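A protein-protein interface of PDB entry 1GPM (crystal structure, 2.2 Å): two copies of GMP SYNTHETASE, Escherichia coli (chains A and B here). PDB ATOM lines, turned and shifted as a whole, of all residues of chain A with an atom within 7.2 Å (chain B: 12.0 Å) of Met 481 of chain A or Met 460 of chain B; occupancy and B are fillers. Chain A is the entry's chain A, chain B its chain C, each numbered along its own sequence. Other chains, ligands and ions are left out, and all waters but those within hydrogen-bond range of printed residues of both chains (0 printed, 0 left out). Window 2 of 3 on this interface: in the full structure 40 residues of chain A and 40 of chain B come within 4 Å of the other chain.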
ATOM      1  N   THR A 477      24.037  -3.668  26.453  1.00  0.00           N
ATOM      2  CA  THR A 477      24.746  -3.443  25.210  1.00  0.00           C
ATOM      3  C   THR A 477      26.018  -2.646  25.453  1.00  0.00           C
ATOM      4  O   THR A 477      25.971  -1.534  25.975  1.00  0.00           O
ATOM      5  CB  THR A 477      23.862  -2.700  24.220  1.00  0.00           C
ATOM      6  OG1 THR A 477      22.584  -3.341  24.171  1.00  0.00           O
ATOM      7  CG2 THR A 477      24.488  -2.718  22.828  1.00  0.00           C
ATOM      8  N   ILE A 478      27.148  -3.264  25.121  1.00  0.00           N
ATOM      9  CA  ILE A 478      28.466  -2.656  25.267  1.00  0.00           C
ATOM     10  C   ILE A 478      28.675  -1.767  24.041  1.00  0.00           C
ATOM     11  O   ILE A 478      28.989  -0.578  24.158  1.00  0.00           O
ATOM     12  CB  ILE A 478      29.564  -3.734  25.297  1.00  0.00           C
ATOM     13  CG1 ILE A 478      29.220  -4.803  26.337  1.00  0.00           C
ATOM     14  CG2 ILE A 478      30.917  -3.104  25.590  1.00  0.00           C
ATOM     15  CD1 ILE A 478      29.069  -4.281  27.749  1.00  0.00           C
ATOM     16  N   ASP A 479      28.487  -2.363  22.869  1.00  0.00           N
ATOM     17  CA  ASP A 479      28.607  -1.670  21.596  1.00  0.00           C
ATOM     18  C   ASP A 479      27.680  -2.366  20.612  1.00  0.00           C
ATOM     19  O   ASP A 479      27.049  -3.373  20.940  1.00  0.00           O
ATOM     20  CB  ASP A 479      30.051  -1.666  21.081  1.00  0.00           C
ATOM     21  CG  ASP A 479      30.638  -3.053  20.959  1.00  0.00           C
ATOM     22  OD1 ASP A 479      30.219  -3.799  20.053  1.00  0.00           O
ATOM     23  OD2 ASP A 479      31.527  -3.393  21.764  1.00  0.00           O
ATOM     24  N   PHE A 480      27.636  -1.864  19.389  1.00  0.00           N
ATOM     25  CA  PHE A 480      26.751  -2.412  18.368  1.00  0.00           C
ATOM     26  C   PHE A 480      27.136  -3.794  17.836  1.00  0.00           C
ATOM     27  O   PHE A 480      26.612  -4.250  16.819  1.00  0.00           O
ATOM     28  CB  PHE A 480      26.582  -1.384  17.247  1.00  0.00           C
ATOM     29  CG  PHE A 480      26.211  -0.011  17.751  1.00  0.00           C
ATOM     30  CD1 PHE A 480      24.880   0.319  17.998  1.00  0.00           C
ATOM     31  CD2 PHE A 480      27.200   0.928  18.044  1.00  0.00           C
ATOM     32  CE1 PHE A 480      24.541   1.566  18.534  1.00  0.00           C
ATOM     33  CE2 PHE A 480      26.871   2.173  18.579  1.00  0.00           C
ATOM     34  CZ  PHE A 480      25.538   2.492  18.825  1.00  0.00           C
ATOM     35  N   MET A 481      27.990  -4.487  18.579  1.00  0.00           N
ATOM     36  CA  MET A 481      28.436  -5.822  18.219  1.00  0.00           C
ATOM     37  C   MET A 481      28.646  -6.671  19.476  1.00  0.00           C
ATOM     38  O   MET A 481      28.840  -7.885  19.391  1.00  0.00           O
ATOM     39  CB  MET A 481      29.724  -5.740  17.395  1.00  0.00           C
ATOM     40  CG  MET A 481      30.288  -7.086  16.981  1.00  0.00           C
ATOM     41  SD  MET A 481      31.567  -6.917  15.744  1.00  0.00           S
ATOM     42  CE  MET A 481      30.650  -7.382  14.260  1.00  0.00           C
ATOM     43  N   THR A 482      28.515  -6.044  20.641  1.00  0.00           N
ATOM     44  CA  THR A 482      28.698  -6.744  21.903  1.00  0.00           C
ATOM     45  C   THR A 482      27.674  -6.322  22.953  1.00  0.00           C
ATOM     46  O   THR A 482      27.468  -5.131  23.194  1.00  0.00           O
ATOM     47  CB  THR A 482      30.134  -6.530  22.444  1.00  0.00           C
ATOM     48  OG1 THR A 482      31.080  -7.098  21.527  1.00  0.00           O
ATOM     49  CG2 THR A 482      30.311  -7.189  23.805  1.00  0.00           C
ATOM     50  N   ALA A 483      27.016  -7.310  23.555  1.00  0.00           N
ATOM     51  CA  ALA A 483      26.012  -7.081  24.596  1.00  0.00           C
ATOM     52  C   ALA A 483      26.032  -8.280  25.533  1.00  0.00           C
ATOM     53  O   ALA A 483      26.117  -9.413  25.081  1.00  0.00           O
ATOM     54  CB  ALA A 483      24.625  -6.910  23.975  1.00  0.00           C
ATOM     55  N   LYS A 517      26.137 -11.619  23.435  1.00  0.00           N
ATOM     56  CA  LYS A 517      26.438 -11.183  22.085  1.00  0.00           C
ATOM     57  C   LYS A 517      27.882 -10.698  22.052  1.00  0.00           C
ATOM     58  O   LYS A 517      28.236  -9.727  22.732  1.00  0.00           O
ATOM     59  CB  LYS A 517      25.505 -10.062  21.632  1.00  0.00           C
ATOM     60  CG  LYS A 517      25.752  -9.651  20.190  1.00  0.00           C
ATOM     61  CD  LYS A 517      24.797  -8.587  19.736  1.00  0.00           C
ATOM     62  CE  LYS A 517      25.187  -8.092  18.350  1.00  0.00           C
ATOM     63  NZ  LYS A 517      24.279  -7.012  17.845  1.00  0.00           N
ATOM     64  N   PRO A 518      28.761 -11.456  21.387  1.00  0.00           N
ATOM     65  CA  PRO A 518      28.436 -12.708  20.701  1.00  0.00           C
ATOM     66  C   PRO A 518      28.457 -13.853  21.728  1.00  0.00           C
ATOM     67  O   PRO A 518      28.665 -13.616  22.922  1.00  0.00           O
ATOM     68  CB  PRO A 518      29.576 -12.827  19.690  1.00  0.00           C
ATOM     69  CG  PRO A 518      30.737 -12.312  20.466  1.00  0.00           C
ATOM     70  CD  PRO A 518      30.165 -11.072  21.136  1.00  0.00           C
ATOM     71  N   PRO A 519      28.244 -15.104  21.286  1.00  0.00           N
ATOM     72  CA  PRO A 519      27.987 -15.571  19.924  1.00  0.00           C
ATOM     73  C   PRO A 519      26.533 -15.504  19.468  1.00  0.00           C
ATOM     74  O   PRO A 519      26.221 -15.873  18.333  1.00  0.00           O
ATOM     75  CB  PRO A 519      28.500 -17.002  19.961  1.00  0.00           C
ATOM     76  CG  PRO A 519      28.181 -17.419  21.349  1.00  0.00           C
ATOM     77  CD  PRO A 519      28.597 -16.235  22.163  1.00  0.00           C
ATOM     78  N   ALA A 520      25.638 -15.054  20.339  1.00  0.00           N
ATOM     79  CA  ALA A 520      24.234 -14.951  19.958  1.00  0.00           C
ATOM     80  C   ALA A 520      23.891 -13.485  19.715  1.00  0.00           C
ATOM     81  O   ALA A 520      24.692 -12.602  20.010  1.00  0.00           O
ATOM     82  CB  ALA A 520      23.348 -15.523  21.043  1.00  0.00           C
ATOM     83  N   THR A 521      22.732 -13.239  19.116  1.00  0.00           N
ATOM     84  CA  THR A 521      22.265 -11.883  18.862  1.00  0.00           C
ATOM     85  C   THR A 521      21.304 -11.518  19.988  1.00  0.00           C
ATOM     86  O   THR A 521      20.905 -12.390  20.786  1.00  0.00           O
ATOM     87  CB  THR A 521      21.525 -11.779  17.515  1.00  0.00           C
ATOM     88  OG1 THR A 521      20.527 -12.803  17.435  1.00  0.00           O
ATOM     89  CG2 THR A 521      22.499 -11.929  16.340  1.00  0.00           C
ATOM     90  N   SER B 456      16.856 -20.024  16.225  1.00  0.00           N
ATOM     91  CA  SER B 456      17.296 -18.699  16.631  1.00  0.00           C
ATOM     92  C   SER B 456      18.420 -18.272  15.678  1.00  0.00           C
ATOM     93  O   SER B 456      19.085 -19.122  15.085  1.00  0.00           O
ATOM     94  CB  SER B 456      17.814 -18.780  18.070  1.00  0.00           C
ATOM     95  OG  SER B 456      18.217 -17.519  18.561  1.00  0.00           O
ATOM     96  N   VAL B 457      18.652 -16.965  15.567  1.00  0.00           N
ATOM     97  CA  VAL B 457      19.688 -16.392  14.689  1.00  0.00           C
ATOM     98  C   VAL B 457      20.963 -16.049  15.462  1.00  0.00           C
ATOM     99  O   VAL B 457      20.943 -16.024  16.697  1.00  0.00           O
ATOM    100  CB  VAL B 457      19.222 -15.050  14.095  1.00  0.00           C
ATOM    101  CG1 VAL B 457      20.002 -14.724  12.854  1.00  0.00           C
ATOM    102  CG2 VAL B 457      17.747 -15.065  13.826  1.00  0.00           C
ATOM    103  N   GLY B 458      22.068 -15.792  14.757  1.00  0.00           N
ATOM    104  CA  GLY B 458      23.263 -15.372  15.469  1.00  0.00           C
ATOM    105  C   GLY B 458      24.710 -15.778  15.241  1.00  0.00           C
ATOM    106  O   GLY B 458      25.593 -14.921  15.351  1.00  0.00           O
ATOM    107  N   VAL B 459      24.978 -17.037  14.912  1.00  0.00           N
ATOM    108  CA  VAL B 459      26.368 -17.497  14.780  1.00  0.00           C
ATOM    109  C   VAL B 459      27.277 -16.776  13.769  1.00  0.00           C
ATOM    110  O   VAL B 459      27.537 -17.273  12.665  1.00  0.00           O
ATOM    111  CB  VAL B 459      26.459 -19.030  14.584  1.00  0.00           C
ATOM    112  CG1 VAL B 459      27.777 -19.531  15.152  1.00  0.00           C
ATOM    113  CG2 VAL B 459      25.289 -19.731  15.271  1.00  0.00           C
ATOM    114  N   MET B 460      27.851 -15.662  14.222  1.00  0.00           N
ATOM    115  CA  MET B 460      28.742 -14.821  13.421  1.00  0.00           C
ATOM    116  C   MET B 460      29.878 -15.533  12.679  1.00  0.00           C
ATOM    117  O   MET B 460      29.971 -15.454  11.448  1.00  0.00           O
ATOM    118  CB  MET B 460      29.329 -13.704  14.296  1.00  0.00           C
ATOM    119  CG  MET B 460      30.295 -12.770  13.563  1.00  0.00           C
ATOM    120  SD  MET B 460      31.072 -11.549  14.640  1.00  0.00           S
ATOM    121  CE  MET B 460      32.328 -10.881  13.554  1.00  0.00           C
ATOM    122  N   GLY B 461      30.762 -16.179  13.435  1.00  0.00           N
ATOM    123  CA  GLY B 461      31.897 -16.869  12.844  1.00  0.00           C
ATOM    124  C   GLY B 461      31.544 -17.946  11.837  1.00  0.00           C
ATOM    125  O   GLY B 461      32.239 -18.124  10.830  1.00  0.00           O
ATOM    126  N   ASP B 462      30.472 -18.678  12.114  1.00  0.00           N
ATOM    127  CA  ASP B 462      30.032 -19.745  11.231  1.00  0.00           C
ATOM    128  C   ASP B 462      29.469 -19.219   9.933  1.00  0.00           C
ATOM    129  O   ASP B 462      29.682 -19.808   8.872  1.00  0.00           O
ATOM    130  CB  ASP B 462      28.975 -20.607  11.918  1.00  0.00           C
ATOM    131  CG  ASP B 462      29.560 -21.511  12.974  1.00  0.00           C
ATOM    132  OD1 ASP B 462      30.338 -21.012  13.816  1.00  0.00           O
ATOM    133  OD2 ASP B 462      29.274 -22.725  12.941  1.00  0.00           O
ATOM    134  N   GLY B 463      28.808 -18.071  10.010  1.00  0.00           N
ATOM    135  CA  GLY B 463      28.180 -17.514   8.830  1.00  0.00           C
ATOM    136  C   GLY B 463      26.814 -18.170   8.749  1.00  0.00           C
ATOM    137  O   GLY B 463      26.041 -17.943   7.818  1.00  0.00           O
ATOM    138  N   ARG B 464      26.530 -18.988   9.761  1.00  0.00           N
ATOM    139  CA  ARG B 464      25.281 -19.717   9.884  1.00  0.00           C
ATOM    140  C   ARG B 464      24.323 -18.828  10.662  1.00  0.00           C
ATOM    141  O   ARG B 464      24.674 -18.295  11.722  1.00  0.00           O
ATOM    142  CB  ARG B 464      25.528 -21.025  10.639  1.00  0.00           C
ATOM    143  CG  ARG B 464      24.371 -22.003  10.616  1.00  0.00           C
ATOM    144  CD  ARG B 464      24.876 -23.408  10.905  1.00  0.00           C
ATOM    145  NE  ARG B 464      23.823 -24.412  10.783  1.00  0.00           N
ATOM    146  CZ  ARG B 464      24.009 -25.720  10.946  1.00  0.00           C
ATOM    147  NH1 ARG B 464      25.215 -26.190  11.246  1.00  0.00           N
ATOM    148  NH2 ARG B 464      22.985 -26.556  10.813  1.00  0.00           N
ATOM    149  N   LYS B 465      23.119 -18.655  10.135  1.00  0.00           N
ATOM    150  CA  LYS B 465      22.140 -17.807  10.791  1.00  0.00           C
ATOM    151  C   LYS B 465      21.175 -18.513  11.739  1.00  0.00           C
ATOM    152  O   LYS B 465      21.204 -18.268  12.944  1.00  0.00           O
ATOM    153  CB  LYS B 465      21.366 -16.989   9.753  1.00  0.00           C
ATOM    154  CG  LYS B 465      22.240 -16.058   8.933  1.00  0.00           C
ATOM    155  CD  LYS B 465      21.423 -15.373   7.852  1.00  0.00           C
ATOM    156  CE  LYS B 465      22.315 -14.682   6.829  1.00  0.00           C
ATOM    157  NZ  LYS B 465      21.527 -14.109   5.696  1.00  0.00           N
ATOM    158  N   TYR B 466      20.353 -19.413  11.208  1.00  0.00           N
ATOM    159  CA  TYR B 466      19.356 -20.102  12.018  1.00  0.00           C
ATOM    160  C   TYR B 466      19.674 -21.499  12.526  1.00  0.00           C
ATOM    161  O   TYR B 466      19.707 -22.462  11.758  1.00  0.00           O
ATOM    162  CB  TYR B 466      18.021 -20.122  11.282  1.00  0.00           C
ATOM    163  CG  TYR B 466      17.589 -18.748  10.866  1.00  0.00           C
ATOM    164  CD1 TYR B 466      17.053 -17.862  11.790  1.00  0.00           C
ATOM    165  CD2 TYR B 466      17.767 -18.308   9.550  1.00  0.00           C
ATOM    166  CE1 TYR B 466      16.709 -16.570  11.418  1.00  0.00           C
ATOM    167  CE2 TYR B 466      17.425 -17.010   9.169  1.00  0.00           C
ATOM    168  CZ  TYR B 466      16.898 -16.150  10.113  1.00  0.00           C
ATOM    169  OH  TYR B 466      16.551 -14.866   9.774  1.00  0.00           O
ATOM    170  N   ASP B 467      19.818 -21.612  13.841  1.00  0.00           N
ATOM    171  CA  ASP B 467      20.092 -22.890  14.476  1.00  0.00           C
ATOM    172  C   ASP B 467      19.154 -23.142  15.640  1.00  0.00           C
ATOM    173  O   ASP B 467      18.346 -22.287  15.990  1.00  0.00           O
ATOM    174  CB  ASP B 467      21.549 -22.991  14.908  1.00  0.00           C
ATOM    175  CG  ASP B 467      22.417 -23.638  13.850  1.00  0.00           C
ATOM    176  OD1 ASP B 467      21.917 -24.548  13.145  1.00  0.00           O
ATOM    177  OD2 ASP B 467      23.597 -23.248  13.725  1.00  0.00           O
ATOM    178  N   ASN B 498      28.378 -20.422  26.708  1.00  0.00           N
ATOM    179  CA  ASN B 498      29.447 -20.069  25.789  1.00  0.00           C
ATOM    180  C   ASN B 498      30.004 -21.339  25.158  1.00  0.00           C
ATOM    181  O   ASN B 498      29.983 -21.485  23.936  1.00  0.00           O
ATOM    182  CB  ASN B 498      30.555 -19.297  26.511  1.00  0.00           C
ATOM    183  CG  ASN B 498      30.259 -17.813  26.618  1.00  0.00           C
ATOM    184  OD1 ASN B 498      29.651 -17.228  25.721  1.00  0.00           O
ATOM    185  ND2 ASN B 498      30.678 -17.195  27.719  1.00  0.00           N
ATOM    186  N   ILE B 501      27.243 -23.147  22.757  1.00  0.00           N
ATOM    187  CA  ILE B 501      27.005 -22.488  21.471  1.00  0.00           C
ATOM    188  C   ILE B 501      28.224 -22.604  20.542  1.00  0.00           C
ATOM    189  O   ILE B 501      28.092 -22.892  19.342  1.00  0.00           O
ATOM    190  CB  ILE B 501      26.621 -20.987  21.682  1.00  0.00           C
ATOM    191  CG1 ILE B 501      25.256 -20.893  22.368  1.00  0.00           C
ATOM    192  CG2 ILE B 501      26.560 -20.245  20.350  1.00  0.00           C
ATOM    193  CD1 ILE B 501      24.919 -19.514  22.905  1.00  0.00           C
ATOM    194  N   ASN B 502      29.408 -22.452  21.126  1.00  0.00           N
ATOM    195  CA  ASN B 502      30.667 -22.509  20.384  1.00  0.00           C
ATOM    196  C   ASN B 502      31.141 -23.898  19.965  1.00  0.00           C
ATOM    197  O   ASN B 502      31.716 -24.064  18.890  1.00  0.00           O
ATOM    198  CB  ASN B 502      31.776 -21.834  21.191  1.00  0.00           C
ATOM    199  CG  ASN B 502      31.527 -20.344  21.401  1.00  0.00           C
ATOM    200  OD1 ASN B 502      31.161 -19.621  20.470  1.00  0.00           O
ATOM    201  ND2 ASN B 502      31.759 -19.873  22.623  1.00  0.00           N
ATOM    202  N   GLU B 503      30.920 -24.890  20.815  1.00  0.00           N
ATOM    203  CA  GLU B 503      31.374 -26.248  20.530  1.00  0.00           C
ATOM    204  C   GLU B 503      30.354 -27.159  19.862  1.00  0.00           C
ATOM    205  O   GLU B 503      30.717 -28.229  19.370  1.00  0.00           O
ATOM    206  CB  GLU B 503      31.910 -26.905  21.804  1.00  0.00           C
ATOM    207  CG  GLU B 503      33.150 -26.227  22.378  1.00  0.00           C
ATOM    208  CD  GLU B 503      33.480 -26.676  23.798  1.00  0.00           C
ATOM    209  OE1 GLU B 503      33.348 -27.879  24.107  1.00  0.00           O
ATOM    210  OE2 GLU B 503      33.877 -25.823  24.623  1.00  0.00           O
ATOM    211  N   VAL B 504      29.089 -26.751  19.822  1.00  0.00           N
ATOM    212  CA  VAL B 504      28.064 -27.592  19.208  1.00  0.00           C
ATOM    213  C   VAL B 504      27.422 -26.962  17.977  1.00  0.00           C
ATOM    214  O   VAL B 504      26.434 -26.222  18.078  1.00  0.00           O
ATOM    215  CB  VAL B 504      26.946 -27.961  20.207  1.00  0.00           C
ATOM    216  CG1 VAL B 504      26.065 -29.049  19.622  1.00  0.00           C
ATOM    217  CG2 VAL B 504      27.540 -28.397  21.534  1.00  0.00           C
ATOM    218  N   ASN B 505      27.971 -27.271  16.810  1.00  0.00           N
ATOM    219  CA  ASN B 505      27.426 -26.747  15.561  1.00  0.00           C
ATOM    220  C   ASN B 505      25.998 -27.253  15.404  1.00  0.00           C
ATOM    221  O   ASN B 505      25.763 -28.453  15.227  1.00  0.00           O
ATOM    222  CB  ASN B 505      28.275 -27.180  14.359  1.00  0.00           C
ATOM    223  CG  ASN B 505      29.694 -26.664  14.438  1.00  0.00           C
ATOM    224  OD1 ASN B 505      29.983 -25.723  15.175  1.00  0.00           O
ATOM    225  ND2 ASN B 505      30.595 -27.295  13.700  1.00  0.00           N
ATOM    226  N   GLY B 506      25.050 -26.331  15.477  1.00  0.00           N
ATOM    227  CA  GLY B 506      23.660 -26.702  15.358  1.00  0.00           C
ATOM    228  C   GLY B 506      22.877 -26.009  16.449  1.00  0.00           C
ATOM    229  O   GLY B 506      21.640 -25.977  16.408  1.00  0.00           O
ATOM    230  N   ILE B 507      23.593 -25.472  17.440  1.00  0.00           N
ATOM    231  CA  ILE B 507      22.958 -24.771  18.548  1.00  0.00           C
ATOM    232  C   ILE B 507      23.387 -23.307  18.537  1.00  0.00           C
ATOM    233  O   ILE B 507      24.573 -22.998  18.636  1.00  0.00           O
ATOM    234  CB  ILE B 507      23.309 -25.430  19.893  1.00  0.00           C
ATOM    235  CG1 ILE B 507      22.695 -26.826  19.951  1.00  0.00           C
ATOM    236  CG2 ILE B 507      22.798 -24.592  21.063  1.00  0.00           C
ATOM    237  CD1 ILE B 507      23.160 -27.638  21.139  1.00  0.00           C
ATOM    238  N   SER B 508      22.421 -22.412  18.355  1.00  0.00           N
ATOM    239  CA  SER B 508      22.702 -20.982  18.315  1.00  0.00           C
ATOM    240  C   SER B 508      22.413 -20.268  19.637  1.00  0.00           C
ATOM    241  O   SER B 508      22.958 -19.195  19.895  1.00  0.00           O
ATOM    242  CB  SER B 508      21.898 -20.319  17.191  1.00  0.00           C
ATOM    243  OG  SER B 508      20.499 -20.518  17.357  1.00  0.00           O
ATOM    244  N   ARG B 509      21.595 -20.875  20.495  1.00  0.00           N
ATOM    245  CA  ARG B 509      21.252 -20.225  21.749  1.00  0.00           C
ATOM    246  C   ARG B 509      20.947 -21.185  22.883  1.00  0.00           C
ATOM    247  O   ARG B 509      20.400 -22.270  22.678  1.00  0.00           O
ATOM    248  CB  ARG B 509      20.050 -19.307  21.519  1.00  0.00           C
ATOM    249  CG  ARG B 509      19.806 -18.303  22.606  1.00  0.00           C
ATOM    250  CD  ARG B 509      18.734 -17.327  22.211  1.00  0.00           C
ATOM    251  NE  ARG B 509      19.019 -16.640  20.947  1.00  0.00           N
ATOM    252  CZ  ARG B 509      19.201 -15.329  20.828  1.00  0.00           C
ATOM    253  NH1 ARG B 509      19.152 -14.554  21.909  1.00  0.00           N
ATOM    254  NH2 ARG B 509      19.321 -14.784  19.614  1.00  0.00           N
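CE of Met 460 of chain B touches CE of Met 481 of chain A (3.9 Å).
O of Pro 519 of chain A touches N of Val 459 of chain B (3.8 Å).
OD1 of Asn 498 of chain B touches CD of Pro 519 of chain A, 3.8 Å away.
CG2 of Ile 501 of chain B touches CG of Pro 519 of chain A, at 3.4 Å.
Asn 502 of chain B touches Pro 519 of chain A (OD1 to CB, 3.8 Å).
Ala 520 of chain A touches Ser 508 of chain B (CB to O, 3.9 Å).
CG2 of Thr 521 of chain A touches CA of Gly 458 of chain B (3.6 Å).
OD1 of Asp 479 of chain A is in hydrogen-bond range of N of Met 481 of chain A, 2.8 Å away.
O of Ser 456 of chain B sits at hydrogen-bond distance from OG of Ser 508 of chain B (3.0 Å).
The backbone NH (N) of Gly 458 of chain B lies within hydrogen-bond range of the backbone carbonyl oxygen (O) of Lys 465 of chain B, at 3.2 Å.
N of Val 459 of chain B sits at hydrogen-bond distance from O of Arg 464 of chain B.
The side-chain hydroxyl (OG) of Ser 508 of chain B is in hydrogen-bond range of the backbone carbonyl oxygen (O) of Asp 467 of chain B (3.1 Å).
O of Asn 498 of chain B is in hydrogen-bond range of ND2 of Asn 502 of chain B, at 2.7 Å.
Hydrophobic or aromatic side chains of chain B within 4 Å of the printed part of chain A: Met 460 and Ile 501.
Along chain B the printed residues that touch a printed residue of chain A span positions 457 to 509.
Printed residues of chain A that touch a printed residue of chain B: Met 481, Pro 519, Ala 520 and Thr 521.
Hydrophobic or aromatic side chains of chain A within 4 Å of the printed part of chain B: Met 481, Pro 519 and Ala 520.
Among the printed residues, 10 pairs touch across the chains.
OG1 of Thr 521 of chain A is in hydrogen-bond range of O of Val 457 of chain B (3.3 Å).
The guanidinium group (NH1) of Arg 509 of chain B lies within hydrogen-bond range of the backbone carbonyl oxygen (O) of Thr 521 of chain A, at 3.0 Å.
The backbone carbonyl oxygen of Pro 519 of chain A lies close to the backbone carbonyl oxygen of Gly 458 of chain B, at 3.2 Å.
No position is printed for both chains.
Of the 10 pairs that touch across the chains among the printed residues, none has its exchanged pair printed and touching as well.
Thr 477 of chain A touches none of the printed residues of chain B.
Met 481 of chain A touches just one residue of chain B: Met 460 (3.9 Å).
No residue of chain B comes within 4 Å of Thr 482 of chain A.
No residue of chain B comes within 4 Å of Lys 517 of chain A.
No residue of chain B comes within 4 Å of Pro 518 of chain A.
Of the printed residues of chain B, Thr 521 of chain A touches Val 457, Gly 458 and Arg 509.
Printed residues of chain A within 4 Å of Gly 458 of chain B: Pro 519 and Thr 521.
Of the printed residues of chain A, Met 460 of chain B touches Met 481.
Lys 465 of chain B touches none of the printed residues of chain A.
Printed residues of chain A within 4 Å of Asn 498 of chain B: Pro 519 (3.8 Å).
The nearest residue of chain B that does not touch Met 481 of chain A is Gly 458 of chain B (8.7 Å).
The nearest residue of chain A that does not touch Met 460 of chain B is Pro 519 of chain A (4.4 Å).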
